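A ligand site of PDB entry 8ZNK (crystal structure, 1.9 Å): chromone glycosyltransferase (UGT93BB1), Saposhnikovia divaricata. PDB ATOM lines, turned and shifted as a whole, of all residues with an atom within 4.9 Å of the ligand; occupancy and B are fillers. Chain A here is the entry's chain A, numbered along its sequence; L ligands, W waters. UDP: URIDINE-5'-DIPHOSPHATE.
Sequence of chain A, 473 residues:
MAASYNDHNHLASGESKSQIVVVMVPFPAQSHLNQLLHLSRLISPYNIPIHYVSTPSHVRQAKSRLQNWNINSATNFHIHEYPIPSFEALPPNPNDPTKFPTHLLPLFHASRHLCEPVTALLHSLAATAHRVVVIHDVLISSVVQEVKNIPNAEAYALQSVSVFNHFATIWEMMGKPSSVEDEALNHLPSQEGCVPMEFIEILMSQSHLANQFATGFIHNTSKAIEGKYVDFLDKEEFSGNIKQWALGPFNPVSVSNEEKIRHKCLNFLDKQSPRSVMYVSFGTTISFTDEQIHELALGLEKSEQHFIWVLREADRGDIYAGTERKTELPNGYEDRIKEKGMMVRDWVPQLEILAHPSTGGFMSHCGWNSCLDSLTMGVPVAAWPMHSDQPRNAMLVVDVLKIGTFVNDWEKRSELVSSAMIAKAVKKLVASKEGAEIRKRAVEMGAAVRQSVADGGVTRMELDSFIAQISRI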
ATOM      1  N   GLN A  30      -2.921  22.812   1.724  1.00  0.00           N
ATOM      2  CA  GLN A  30      -3.564  22.391   0.477  1.00  0.00           C
ATOM      3  C   GLN A  30      -3.341  23.373  -0.669  1.00  0.00           C
ATOM      4  O   GLN A  30      -2.903  22.973  -1.756  1.00  0.00           O
ATOM      5  CB  GLN A  30      -5.068  22.205   0.683  1.00  0.00           C
ATOM      6  CG  GLN A  30      -5.819  21.830  -0.578  1.00  0.00           C
ATOM      7  CD  GLN A  30      -5.226  20.599  -1.266  1.00  0.00           C
ATOM      8  OE1 GLN A  30      -4.768  19.667  -0.600  1.00  0.00           O
ATOM      9  NE2 GLN A  30      -5.250  20.591  -2.588  1.00  0.00           N
ATOM     10  N   SER A  31      -3.702  24.648  -0.469  1.00  0.00           N
ATOM     11  CA  SER A  31      -3.634  25.619  -1.555  1.00  0.00           C
ATOM     12  C   SER A  31      -2.208  25.825  -2.019  1.00  0.00           C
ATOM     13  O   SER A  31      -1.959  26.025  -3.220  1.00  0.00           O
ATOM     14  CB  SER A  31      -4.260  26.952  -1.118  1.00  0.00           C
ATOM     15  OG  SER A  31      -3.451  27.609  -0.160  1.00  0.00           O
ATOM     16  N   ASN A  34      -1.099  22.714  -4.044  1.00  0.00           N
ATOM     17  CA  ASN A  34      -1.756  22.665  -5.342  1.00  0.00           C
ATOM     18  C   ASN A  34      -1.234  23.745  -6.280  1.00  0.00           C
ATOM     19  O   ASN A  34      -1.090  23.497  -7.486  1.00  0.00           O
ATOM     20  CB  ASN A  34      -3.280  22.794  -5.172  1.00  0.00           C
ATOM     21  CG  ASN A  34      -4.045  22.497  -6.459  1.00  0.00           C
ATOM     22  OD1 ASN A  34      -4.058  21.374  -6.949  1.00  0.00           O
ATOM     23  ND2 ASN A  34      -4.650  23.547  -7.034  1.00  0.00           N
ATOM     24  N   GLN A  67      -6.667  18.216  -9.431  1.00  0.00           N
ATOM     25  CA  GLN A  67      -7.676  18.142 -10.472  1.00  0.00           C
ATOM     26  C   GLN A  67      -7.175  18.849 -11.716  1.00  0.00           C
ATOM     27  O   GLN A  67      -6.372  19.785 -11.635  1.00  0.00           O
ATOM     28  CB  GLN A  67      -9.042  18.759 -10.033  1.00  0.00           C
ATOM     29  CG  GLN A  67      -9.607  18.108  -8.767  1.00  0.00           C
ATOM     30  CD  GLN A  67     -10.563  19.027  -8.016  1.00  0.00           C
ATOM     31  OE1 GLN A  67     -10.776  20.184  -8.391  1.00  0.00           O
ATOM     32  NE2 GLN A  67     -11.161  18.509  -6.941  1.00  0.00           N
ATOM     33  N   TYR A 279     -22.906  28.291  -5.591  1.00  0.00           N
ATOM     34  CA  TYR A 279     -21.904  27.380  -5.054  1.00  0.00           C
ATOM     35  C   TYR A 279     -21.330  28.014  -3.796  1.00  0.00           C
ATOM     36  O   TYR A 279     -20.977  29.192  -3.819  1.00  0.00           O
ATOM     37  CB  TYR A 279     -20.809  27.102  -6.090  1.00  0.00           C
ATOM     38  CG  TYR A 279     -19.609  26.325  -5.592  1.00  0.00           C
ATOM     39  CD1 TYR A 279     -19.719  24.982  -5.220  1.00  0.00           C
ATOM     40  CD2 TYR A 279     -18.358  26.921  -5.493  1.00  0.00           C
ATOM     41  CE1 TYR A 279     -18.608  24.253  -4.762  1.00  0.00           C
ATOM     42  CE2 TYR A 279     -17.255  26.223  -5.031  1.00  0.00           C
ATOM     43  CZ  TYR A 279     -17.378  24.892  -4.676  1.00  0.00           C
ATOM     44  OH  TYR A 279     -16.272  24.215  -4.226  1.00  0.00           O
ATOM     45  N   SER A 281     -18.593  27.527  -0.629  1.00  0.00           N
ATOM     46  CA  SER A 281     -17.431  26.737  -0.220  1.00  0.00           C
ATOM     47  C   SER A 281     -16.389  27.674   0.372  1.00  0.00           C
ATOM     48  O   SER A 281     -16.184  28.773  -0.150  1.00  0.00           O
ATOM     49  CB  SER A 281     -16.817  25.966  -1.399  1.00  0.00           C
ATOM     50  OG  SER A 281     -15.620  25.306  -1.002  1.00  0.00           O
ATOM     51  N   PHE A 282     -15.717  27.237   1.424  1.00  0.00           N
ATOM     52  CA  PHE A 282     -14.846  28.101   2.207  1.00  0.00           C
ATOM     53  C   PHE A 282     -13.434  27.529   2.318  1.00  0.00           C
ATOM     54  O   PHE A 282     -12.762  27.674   3.341  1.00  0.00           O
ATOM     55  CB  PHE A 282     -15.462  28.352   3.578  1.00  0.00           C
ATOM     56  CG  PHE A 282     -16.824  28.983   3.500  1.00  0.00           C
ATOM     57  CD1 PHE A 282     -16.953  30.362   3.366  1.00  0.00           C
ATOM     58  CD2 PHE A 282     -17.977  28.204   3.515  1.00  0.00           C
ATOM     59  CE1 PHE A 282     -18.196  30.958   3.284  1.00  0.00           C
ATOM     60  CE2 PHE A 282     -19.225  28.794   3.420  1.00  0.00           C
ATOM     61  CZ  PHE A 282     -19.336  30.176   3.304  1.00  0.00           C
ATOM     62  N   GLY A 283     -12.957  26.896   1.242  1.00  0.00           N
ATOM     63  CA  GLY A 283     -11.567  26.476   1.208  1.00  0.00           C
ATOM     64  C   GLY A 283     -11.244  25.419   2.248  1.00  0.00           C
ATOM     65  O   GLY A 283     -12.085  24.581   2.614  1.00  0.00           O
ATOM     66  N   THR A 284     -10.030  25.493   2.775  1.00  0.00           N
ATOM     67  CA  THR A 284      -9.546  24.497   3.717  1.00  0.00           C
ATOM     68  C   THR A 284      -9.099  25.088   5.041  1.00  0.00           C
ATOM     69  O   THR A 284      -8.625  24.346   5.916  1.00  0.00           O
ATOM     70  CB  THR A 284      -8.370  23.721   3.108  1.00  0.00           C
ATOM     71  OG1 THR A 284      -7.294  24.638   2.842  1.00  0.00           O
ATOM     72  CG2 THR A 284      -8.793  23.013   1.818  1.00  0.00           C
ATOM     73  N   THR A 285      -9.188  26.400   5.221  1.00  0.00           N
ATOM     74  CA  THR A 285      -8.643  27.034   6.415  1.00  0.00           C
ATOM     75  C   THR A 285      -9.713  27.679   7.286  1.00  0.00           C
ATOM     76  O   THR A 285      -9.370  28.436   8.194  1.00  0.00           O
ATOM     77  CB  THR A 285      -7.595  28.077   6.037  1.00  0.00           C
ATOM     78  OG1 THR A 285      -8.258  29.165   5.381  1.00  0.00           O
ATOM     79  CG2 THR A 285      -6.533  27.493   5.113  1.00  0.00           C
ATOM     80  N   VAL A 310     -20.688  23.106   0.223  1.00  0.00           N
ATOM     81  CA  VAL A 310     -19.552  22.295   0.679  1.00  0.00           C
ATOM     82  C   VAL A 310     -19.376  22.592   2.163  1.00  0.00           C
ATOM     83  O   VAL A 310     -18.805  23.615   2.554  1.00  0.00           O
ATOM     84  CB  VAL A 310     -18.281  22.602  -0.104  1.00  0.00           C
ATOM     85  CG1 VAL A 310     -17.142  21.657   0.327  1.00  0.00           C
ATOM     86  CG2 VAL A 310     -18.529  22.481  -1.615  1.00  0.00           C
ATOM     87  N   ARG A 312     -17.579  21.298   5.212  1.00  0.00           N
ATOM     88  CA  ARG A 312     -16.465  20.389   5.500  1.00  0.00           C
ATOM     89  C   ARG A 312     -15.494  21.056   6.454  1.00  0.00           C
ATOM     90  O   ARG A 312     -15.072  22.175   6.205  1.00  0.00           O
ATOM     91  CB  ARG A 312     -15.755  19.986   4.194  1.00  0.00           C
ATOM     92  CG  ARG A 312     -14.745  18.848   4.363  1.00  0.00           C
ATOM     93  CD  ARG A 312     -13.831  18.658   3.118  1.00  0.00           C
ATOM     94  NE  ARG A 312     -13.036  19.857   2.829  1.00  0.00           N
ATOM     95  CZ  ARG A 312     -13.227  20.639   1.777  1.00  0.00           C
ATOM     96  NH1 ARG A 312     -14.133  20.366   0.864  1.00  0.00           N
ATOM     97  NH2 ARG A 312     -12.472  21.726   1.638  1.00  0.00           N
ATOM     98  N   ASP A 346     -17.352  16.490   1.578  1.00  0.00           N
ATOM     99  CA  ASP A 346     -16.055  15.960   1.156  1.00  0.00           C
ATOM    100  C   ASP A 346     -15.399  16.935   0.186  1.00  0.00           C
ATOM    101  O   ASP A 346     -15.758  18.117   0.086  1.00  0.00           O
ATOM    102  CB  ASP A 346     -16.197  14.572   0.542  1.00  0.00           C
ATOM    103  CG  ASP A 346     -17.353  14.490  -0.435  1.00  0.00           C
ATOM    104  OD1 ASP A 346     -17.617  15.482  -1.143  1.00  0.00           O
ATOM    105  OD2 ASP A 346     -17.956  13.399  -0.550  1.00  0.00           O
ATOM    106  N   TRP A 347     -14.433  16.426  -0.569  1.00  0.00           N
ATOM    107  CA  TRP A 347     -13.639  17.227  -1.498  1.00  0.00           C
ATOM    108  C   TRP A 347     -14.291  17.205  -2.863  1.00  0.00           C
ATOM    109  O   TRP A 347     -14.581  16.127  -3.399  1.00  0.00           O
ATOM    110  CB  TRP A 347     -12.212  16.678  -1.556  1.00  0.00           C
ATOM    111  CG  TRP A 347     -11.243  17.502  -2.357  1.00  0.00           C
ATOM    112  CD1 TRP A 347     -10.737  17.205  -3.592  1.00  0.00           C
ATOM    113  CD2 TRP A 347     -10.639  18.729  -1.957  1.00  0.00           C
ATOM    114  NE1 TRP A 347      -9.845  18.175  -3.988  1.00  0.00           N
ATOM    115  CE2 TRP A 347      -9.772  19.124  -3.002  1.00  0.00           C
ATOM    116  CE3 TRP A 347     -10.728  19.528  -0.819  1.00  0.00           C
ATOM    117  CZ2 TRP A 347      -9.004  20.283  -2.929  1.00  0.00           C
ATOM    118  CZ3 TRP A 347      -9.977  20.686  -0.764  1.00  0.00           C
ATOM    119  CH2 TRP A 347      -9.131  21.057  -1.814  1.00  0.00           C
ATOM    120  N   VAL A 348     -14.552  18.382  -3.431  1.00  0.00           N
ATOM    121  CA  VAL A 348     -15.336  18.467  -4.654  1.00  0.00           C
ATOM    122  C   VAL A 348     -14.463  18.999  -5.789  1.00  0.00           C
ATOM    123  O   VAL A 348     -13.410  19.598  -5.517  1.00  0.00           O
ATOM    124  CB  VAL A 348     -16.580  19.369  -4.462  1.00  0.00           C
ATOM    125  CG1 VAL A 348     -17.404  18.890  -3.273  1.00  0.00           C
ATOM    126  CG2 VAL A 348     -16.179  20.816  -4.296  1.00  0.00           C
ATOM    127  N   GLN A 350     -14.000  21.799  -7.554  1.00  0.00           N
ATOM    128  CA  GLN A 350     -14.418  23.193  -7.477  1.00  0.00           C
ATOM    129  C   GLN A 350     -14.341  23.899  -8.827  1.00  0.00           C
ATOM    130  O   GLN A 350     -15.298  24.554  -9.250  1.00  0.00           O
ATOM    131  CB  GLN A 350     -13.553  23.944  -6.456  1.00  0.00           C
ATOM    132  CG  GLN A 350     -13.884  25.444  -6.401  1.00  0.00           C
ATOM    133  CD  GLN A 350     -13.423  26.111  -5.114  1.00  0.00           C
ATOM    134  OE1 GLN A 350     -13.974  25.830  -4.061  1.00  0.00           O
ATOM    135  NE2 GLN A 350     -12.476  27.054  -5.206  1.00  0.00           N
ATOM    136  N   LEU A 351     -13.175  23.833  -9.485  1.00  0.00           N
ATOM    137  CA  LEU A 351     -13.031  24.550 -10.758  1.00  0.00           C
ATOM    138  C   LEU A 351     -14.033  24.053 -11.787  1.00  0.00           C
ATOM    139  O   LEU A 351     -14.615  24.851 -12.538  1.00  0.00           O
ATOM    140  CB  LEU A 351     -11.617  24.382 -11.321  1.00  0.00           C
ATOM    141  CG  LEU A 351     -11.168  25.410 -12.387  1.00  0.00           C
ATOM    142  CD1 LEU A 351     -11.308  26.902 -11.958  1.00  0.00           C
ATOM    143  CD2 LEU A 351      -9.772  25.041 -12.932  1.00  0.00           C
ATOM    144  N   HIS A 365     -14.912  32.371   1.049  1.00  0.00           N
ATOM    145  CA  HIS A 365     -14.091  33.083   2.015  1.00  0.00           C
ATOM    146  C   HIS A 365     -13.048  33.961   1.343  1.00  0.00           C
ATOM    147  O   HIS A 365     -12.334  34.694   2.029  1.00  0.00           O
ATOM    148  CB  HIS A 365     -13.405  32.101   2.978  1.00  0.00           C
ATOM    149  CG  HIS A 365     -12.307  31.304   2.352  1.00  0.00           C
ATOM    150  ND1 HIS A 365     -12.433  30.685   1.132  1.00  0.00           N
ATOM    151  CD2 HIS A 365     -11.059  31.013   2.808  1.00  0.00           C
ATOM    152  CE1 HIS A 365     -11.314  30.040   0.851  1.00  0.00           C
ATOM    153  NE2 HIS A 365     -10.464  30.221   1.851  1.00  0.00           N
ATOM    154  N   GLY A 367     -10.247  33.194  -0.116  1.00  0.00           N
ATOM    155  CA  GLY A 367      -8.888  32.737  -0.329  1.00  0.00           C
ATOM    156  C   GLY A 367      -8.504  32.960  -1.783  1.00  0.00           C
ATOM    157  O   GLY A 367      -9.340  32.903  -2.675  1.00  0.00           O
ATOM    158  N   TRP A 368      -7.223  33.271  -2.014  1.00  0.00           N
ATOM    159  CA  TRP A 368      -6.852  33.787  -3.327  1.00  0.00           C
ATOM    160  C   TRP A 368      -7.046  32.755  -4.424  1.00  0.00           C
ATOM    161  O   TRP A 368      -7.427  33.106  -5.549  1.00  0.00           O
ATOM    162  CB  TRP A 368      -5.405  34.295  -3.304  1.00  0.00           C
ATOM    163  CG  TRP A 368      -5.046  35.007  -4.602  1.00  0.00           C
ATOM    164  CD1 TRP A 368      -3.956  34.749  -5.384  1.00  0.00           C
ATOM    165  CD2 TRP A 368      -5.770  36.070  -5.245  1.00  0.00           C
ATOM    166  NE1 TRP A 368      -3.953  35.569  -6.475  1.00  0.00           N
ATOM    167  CE2 TRP A 368      -5.059  36.376  -6.435  1.00  0.00           C
ATOM    168  CE3 TRP A 368      -6.945  36.769  -4.960  1.00  0.00           C
ATOM    169  CZ2 TRP A 368      -5.481  37.376  -7.312  1.00  0.00           C
ATOM    170  CZ3 TRP A 368      -7.389  37.753  -5.853  1.00  0.00           C
ATOM    171  CH2 TRP A 368      -6.644  38.049  -7.018  1.00  0.00           C
ATOM    172  N   ASN A 369      -6.818  31.474  -4.135  1.00  0.00           N
ATOM    173  CA  ASN A 369      -6.940  30.487  -5.201  1.00  0.00           C
ATOM    174  C   ASN A 369      -8.400  30.318  -5.604  1.00  0.00           C
ATOM    175  O   ASN A 369      -8.710  30.138  -6.798  1.00  0.00           O
ATOM    176  CB  ASN A 369      -6.334  29.155  -4.752  1.00  0.00           C
ATOM    177  CG  ASN A 369      -4.829  29.264  -4.614  1.00  0.00           C
ATOM    178  OD1 ASN A 369      -4.099  29.205  -5.590  1.00  0.00           O
ATOM    179  ND2 ASN A 369      -4.386  29.501  -3.377  1.00  0.00           N
ATOM    180  N   SER A 370      -9.314  30.409  -4.638  1.00  0.00           N
ATOM    181  CA  SER A 370     -10.729  30.389  -4.968  1.00  0.00           C
ATOM    182  C   SER A 370     -11.141  31.653  -5.723  1.00  0.00           C
ATOM    183  O   SER A 370     -11.974  31.594  -6.623  1.00  0.00           O
ATOM    184  CB  SER A 370     -11.554  30.228  -3.689  1.00  0.00           C
ATOM    185  OG  SER A 370     -11.442  28.903  -3.170  1.00  0.00           O
ATOM    186  N   ASP A 373     -10.038  30.997  -9.239  1.00  0.00           N
ATOM    187  CA  ASP A 373     -10.995  30.028  -9.772  1.00  0.00           C
ATOM    188  C   ASP A 373     -12.230  30.742 -10.308  1.00  0.00           C
ATOM    189  O   ASP A 373     -12.647  30.535 -11.453  1.00  0.00           O
ATOM    190  CB  ASP A 373     -11.360  29.125  -8.593  1.00  0.00           C
ATOM    191  CG  ASP A 373     -10.483  27.900  -8.452  1.00  0.00           C
ATOM    192  OD1 ASP A 373      -9.323  27.824  -8.950  1.00  0.00           O
ATOM    193  OD2 ASP A 373     -10.848  27.149  -7.529  1.00  0.00           O
ATOM    194  N   GLN A 390      -7.631  37.464   3.092  1.00  0.00           N
ATOM    195  CA  GLN A 390      -8.969  37.412   2.537  1.00  0.00           C
ATOM    196  C   GLN A 390      -9.708  38.751   2.468  1.00  0.00           C
ATOM    197  O   GLN A 390     -10.381  38.990   1.450  1.00  0.00           O
ATOM    198  CB  GLN A 390      -9.792  36.374   3.312  1.00  0.00           C
ATOM    199  CG  GLN A 390      -9.246  34.949   3.115  1.00  0.00           C
ATOM    200  CD  GLN A 390      -9.571  34.026   4.280  1.00  0.00           C
ATOM    201  OE1 GLN A 390     -10.533  34.253   5.017  1.00  0.00           O
ATOM    202  NE2 GLN A 390      -8.762  32.984   4.447  1.00  0.00           N
HETATM  203  N1  UDP L   1     -10.784  23.185  -3.653  1.00  0.00           N
HETATM  204  C2  UDP L   1     -11.187  22.036  -4.309  1.00  0.00           C
HETATM  205  N3  UDP L   1     -12.253  21.392  -3.740  1.00  0.00           N
HETATM  206  C4  UDP L   1     -12.924  21.745  -2.585  1.00  0.00           C
HETATM  207  C5  UDP L   1     -12.440  22.929  -1.945  1.00  0.00           C
HETATM  208  C6  UDP L   1     -11.384  23.568  -2.474  1.00  0.00           C
HETATM  209  O2  UDP L   1     -10.647  21.635  -5.336  1.00  0.00           O
HETATM  210  O4  UDP L   1     -13.854  21.044  -2.194  1.00  0.00           O
HETATM  211  C1' UDP L   1      -9.565  23.873  -4.137  1.00  0.00           C
HETATM  212  C2' UDP L   1      -9.766  25.207  -4.853  1.00  0.00           C
HETATM  213  O2' UDP L   1     -10.009  24.961  -6.217  1.00  0.00           O
HETATM  214  C3' UDP L   1      -8.395  25.859  -4.586  1.00  0.00           C
HETATM  215  C4' UDP L   1      -8.148  25.463  -3.129  1.00  0.00           C
HETATM  216  O4' UDP L   1      -8.792  24.166  -2.986  1.00  0.00           O
HETATM  217  O3' UDP L   1      -7.391  25.279  -5.404  1.00  0.00           O
HETATM  218  C5' UDP L   1      -8.673  26.420  -2.091  1.00  0.00           C
HETATM  219  O5' UDP L   1      -7.706  27.492  -1.986  1.00  0.00           O
HETATM  220  PA  UDP L   1      -8.080  28.915  -1.368  1.00  0.00           P
HETATM  221  O1A UDP L   1      -6.950  29.861  -1.628  1.00  0.00           O
HETATM  222  O2A UDP L   1      -9.453  29.318  -1.788  1.00  0.00           O
HETATM  223  O3A UDP L   1      -8.170  28.680   0.210  1.00  0.00           O
HETATM  224  PB  UDP L   1      -7.491  27.963   1.472  1.00  0.00           P
HETATM  225  O1B UDP L   1      -6.005  28.112   1.435  1.00  0.00           O
HETATM  226  O2B UDP L   1      -8.131  28.690   2.624  1.00  0.00           O
HETATM  227  O3B UDP L   1      -7.924  26.512   1.380  1.00  0.00           O
HETATM  228  O   HOH W   1      -7.846  20.697  -6.342  1.00  0.00           O
HETATM  229  O   HOH W   2      -4.423  25.821   2.051  1.00  0.00           O
HETATM  230  O   HOH W   3      -6.387  22.617  -4.498  1.00  0.00           O
HETATM  231  O   HOH W   4     -14.213  23.759   0.746  1.00  0.00           O
HETATM  232  O   HOH W   5      -7.396  26.180  -7.929  1.00  0.00           O
HETATM  233  O   HOH W   6     -10.597  22.870  -8.216  1.00  0.00           O
HETATM  234  O   HOH W   7      -4.505  26.062  -5.235  1.00  0.00           O
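An oxygen (O2A) of the ligand sits close to the backbone NH (N) of Ser 370 (3.1 Å).
OG of Ser 370 lies within hydrogen-bond range of O2A of the ligand (2.5 Å).
O3B of the ligand is in hydrogen-bond range of N of Thr 284, 2.7 Å away.
O3B of the ligand lies within hydrogen-bond range of OG1 of Thr 284, 2.5 Å away.
OD2 of Asp 373 lies within hydrogen-bond range of O2' of the ligand (2.7 Å).
O4 of the ligand sits at hydrogen-bond distance from N of Val 348 (3.0 Å).
The backbone carbonyl oxygen (O) of Val 348 is in hydrogen-bond range of a nitrogen (N3) of the ligand (2.8 Å).
The side-chain hydroxyl (OG1) of Thr 285 lies within hydrogen-bond range of an oxygen (O2B) of the ligand (2.8 Å).
O2B of the ligand lies within hydrogen-bond range of NE2 of His 365 (2.9 Å).
O1A of the ligand lies within hydrogen-bond range of N of Asn 369 (3.0 Å).
ND2 of Asn 369 is in hydrogen-bond range of O1A of the ligand, at 3.1 Å.
The side-chain hydroxyl (OG) of Ser 31 sits at hydrogen-bond distance from an oxygen (O1B) of the ligand, 3.1 Å away.
The guanidinium group (NH1) of Arg 312 sits at hydrogen-bond distance from an oxygen (O4) of the ligand.
An oxygen (O2') of the ligand sits close to the side-chain amide nitrogen (NE2) of Gln 350.
The side-chain amide oxygen of Gln 67 lies close to an oxygen (O2) of the ligand, at 3.4 Å.
The backbone NH (N) of Trp 368 is in hydrogen-bond range of an oxygen (O1A) of the ligand.
The side-chain hydroxyl (OG) of Ser 370 sits at hydrogen-bond distance from the side-chain amide nitrogen (NE2) of Gln 350.
OD2 of Asp 373 is in hydrogen-bond range of NE2 of Gln 350.
The backbone carbonyl oxygen of Val 348 lies within hydrogen-bond range of the side-chain amide nitrogen of Gln 67, 2.9 Å away.
NE1 of Trp 347 lies close to NE2 of Gln 67 (3.3 Å).
The guanidinium group (NH2) of Arg 312 lies within hydrogen-bond range of the backbone carbonyl oxygen (O) of Gly 283.
The backbone carbonyl oxygen (O) of Asp 346 sits at hydrogen-bond distance from the guanidinium group (NH1) of Arg 312 (2.9 Å).
OE1 of Gln 350 lies within hydrogen-bond range of OH of Tyr 279, at 2.8 Å.
ND2 of Asn 34 touches O3' of the ligand, 3.6 Å away.
Gly 283 touches the ligand (C to O3B, 3.6 Å).
Trp 347 touches the ligand.
C of Gly 367 touches O1A of the ligand (3.5 Å).
Hydrophobic or aromatic side chains that line the ligand: Trp 347, Val 348 and His 365.
16 residues have an atom within 4 Å of the ligand: Ser 31, Asn 34, Gln 67, Gly 283, Thr 284, Thr 285, Arg 312, Trp 347, Val 348, Gln 350, His 365, Gly 367, Trp 368, Asn 369, Ser 370 and Asp 373.
Water W5 bridges an oxygen (O3') of the ligand and the side-chain carboxylate of Asp 373.
Water W2 lies within hydrogen-bond range of O1B of the ligand, N of Ser 31, OG1 of Thr 284 and N of Gln 30.
Water W6 lies within hydrogen-bond range of the side-chain amide oxygen of Gln 67, an oxygen (O2') of the ligand and the backbone NH of Leu 351.
Water W3 lies within hydrogen-bond range of O3' of the ligand (3.0 Å), NE2 of Gln 30 (3.0 Å) and ND2 of Asn 34 (3.2 Å).
Water W7 lies within hydrogen-bond range of O3' of the ligand (3.0 Å), ND2 of Asn 34 (3.1 Å), OD1 of Asn 369 (3.2 Å) and O of Ser 31 (3.2 Å).
Water W4 lies within hydrogen-bond range of the side-chain hydroxyl (OG) of Ser 281, the guanidinium group (NH2) of Arg 312 and the backbone carbonyl oxygen (O) of Gly 283.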
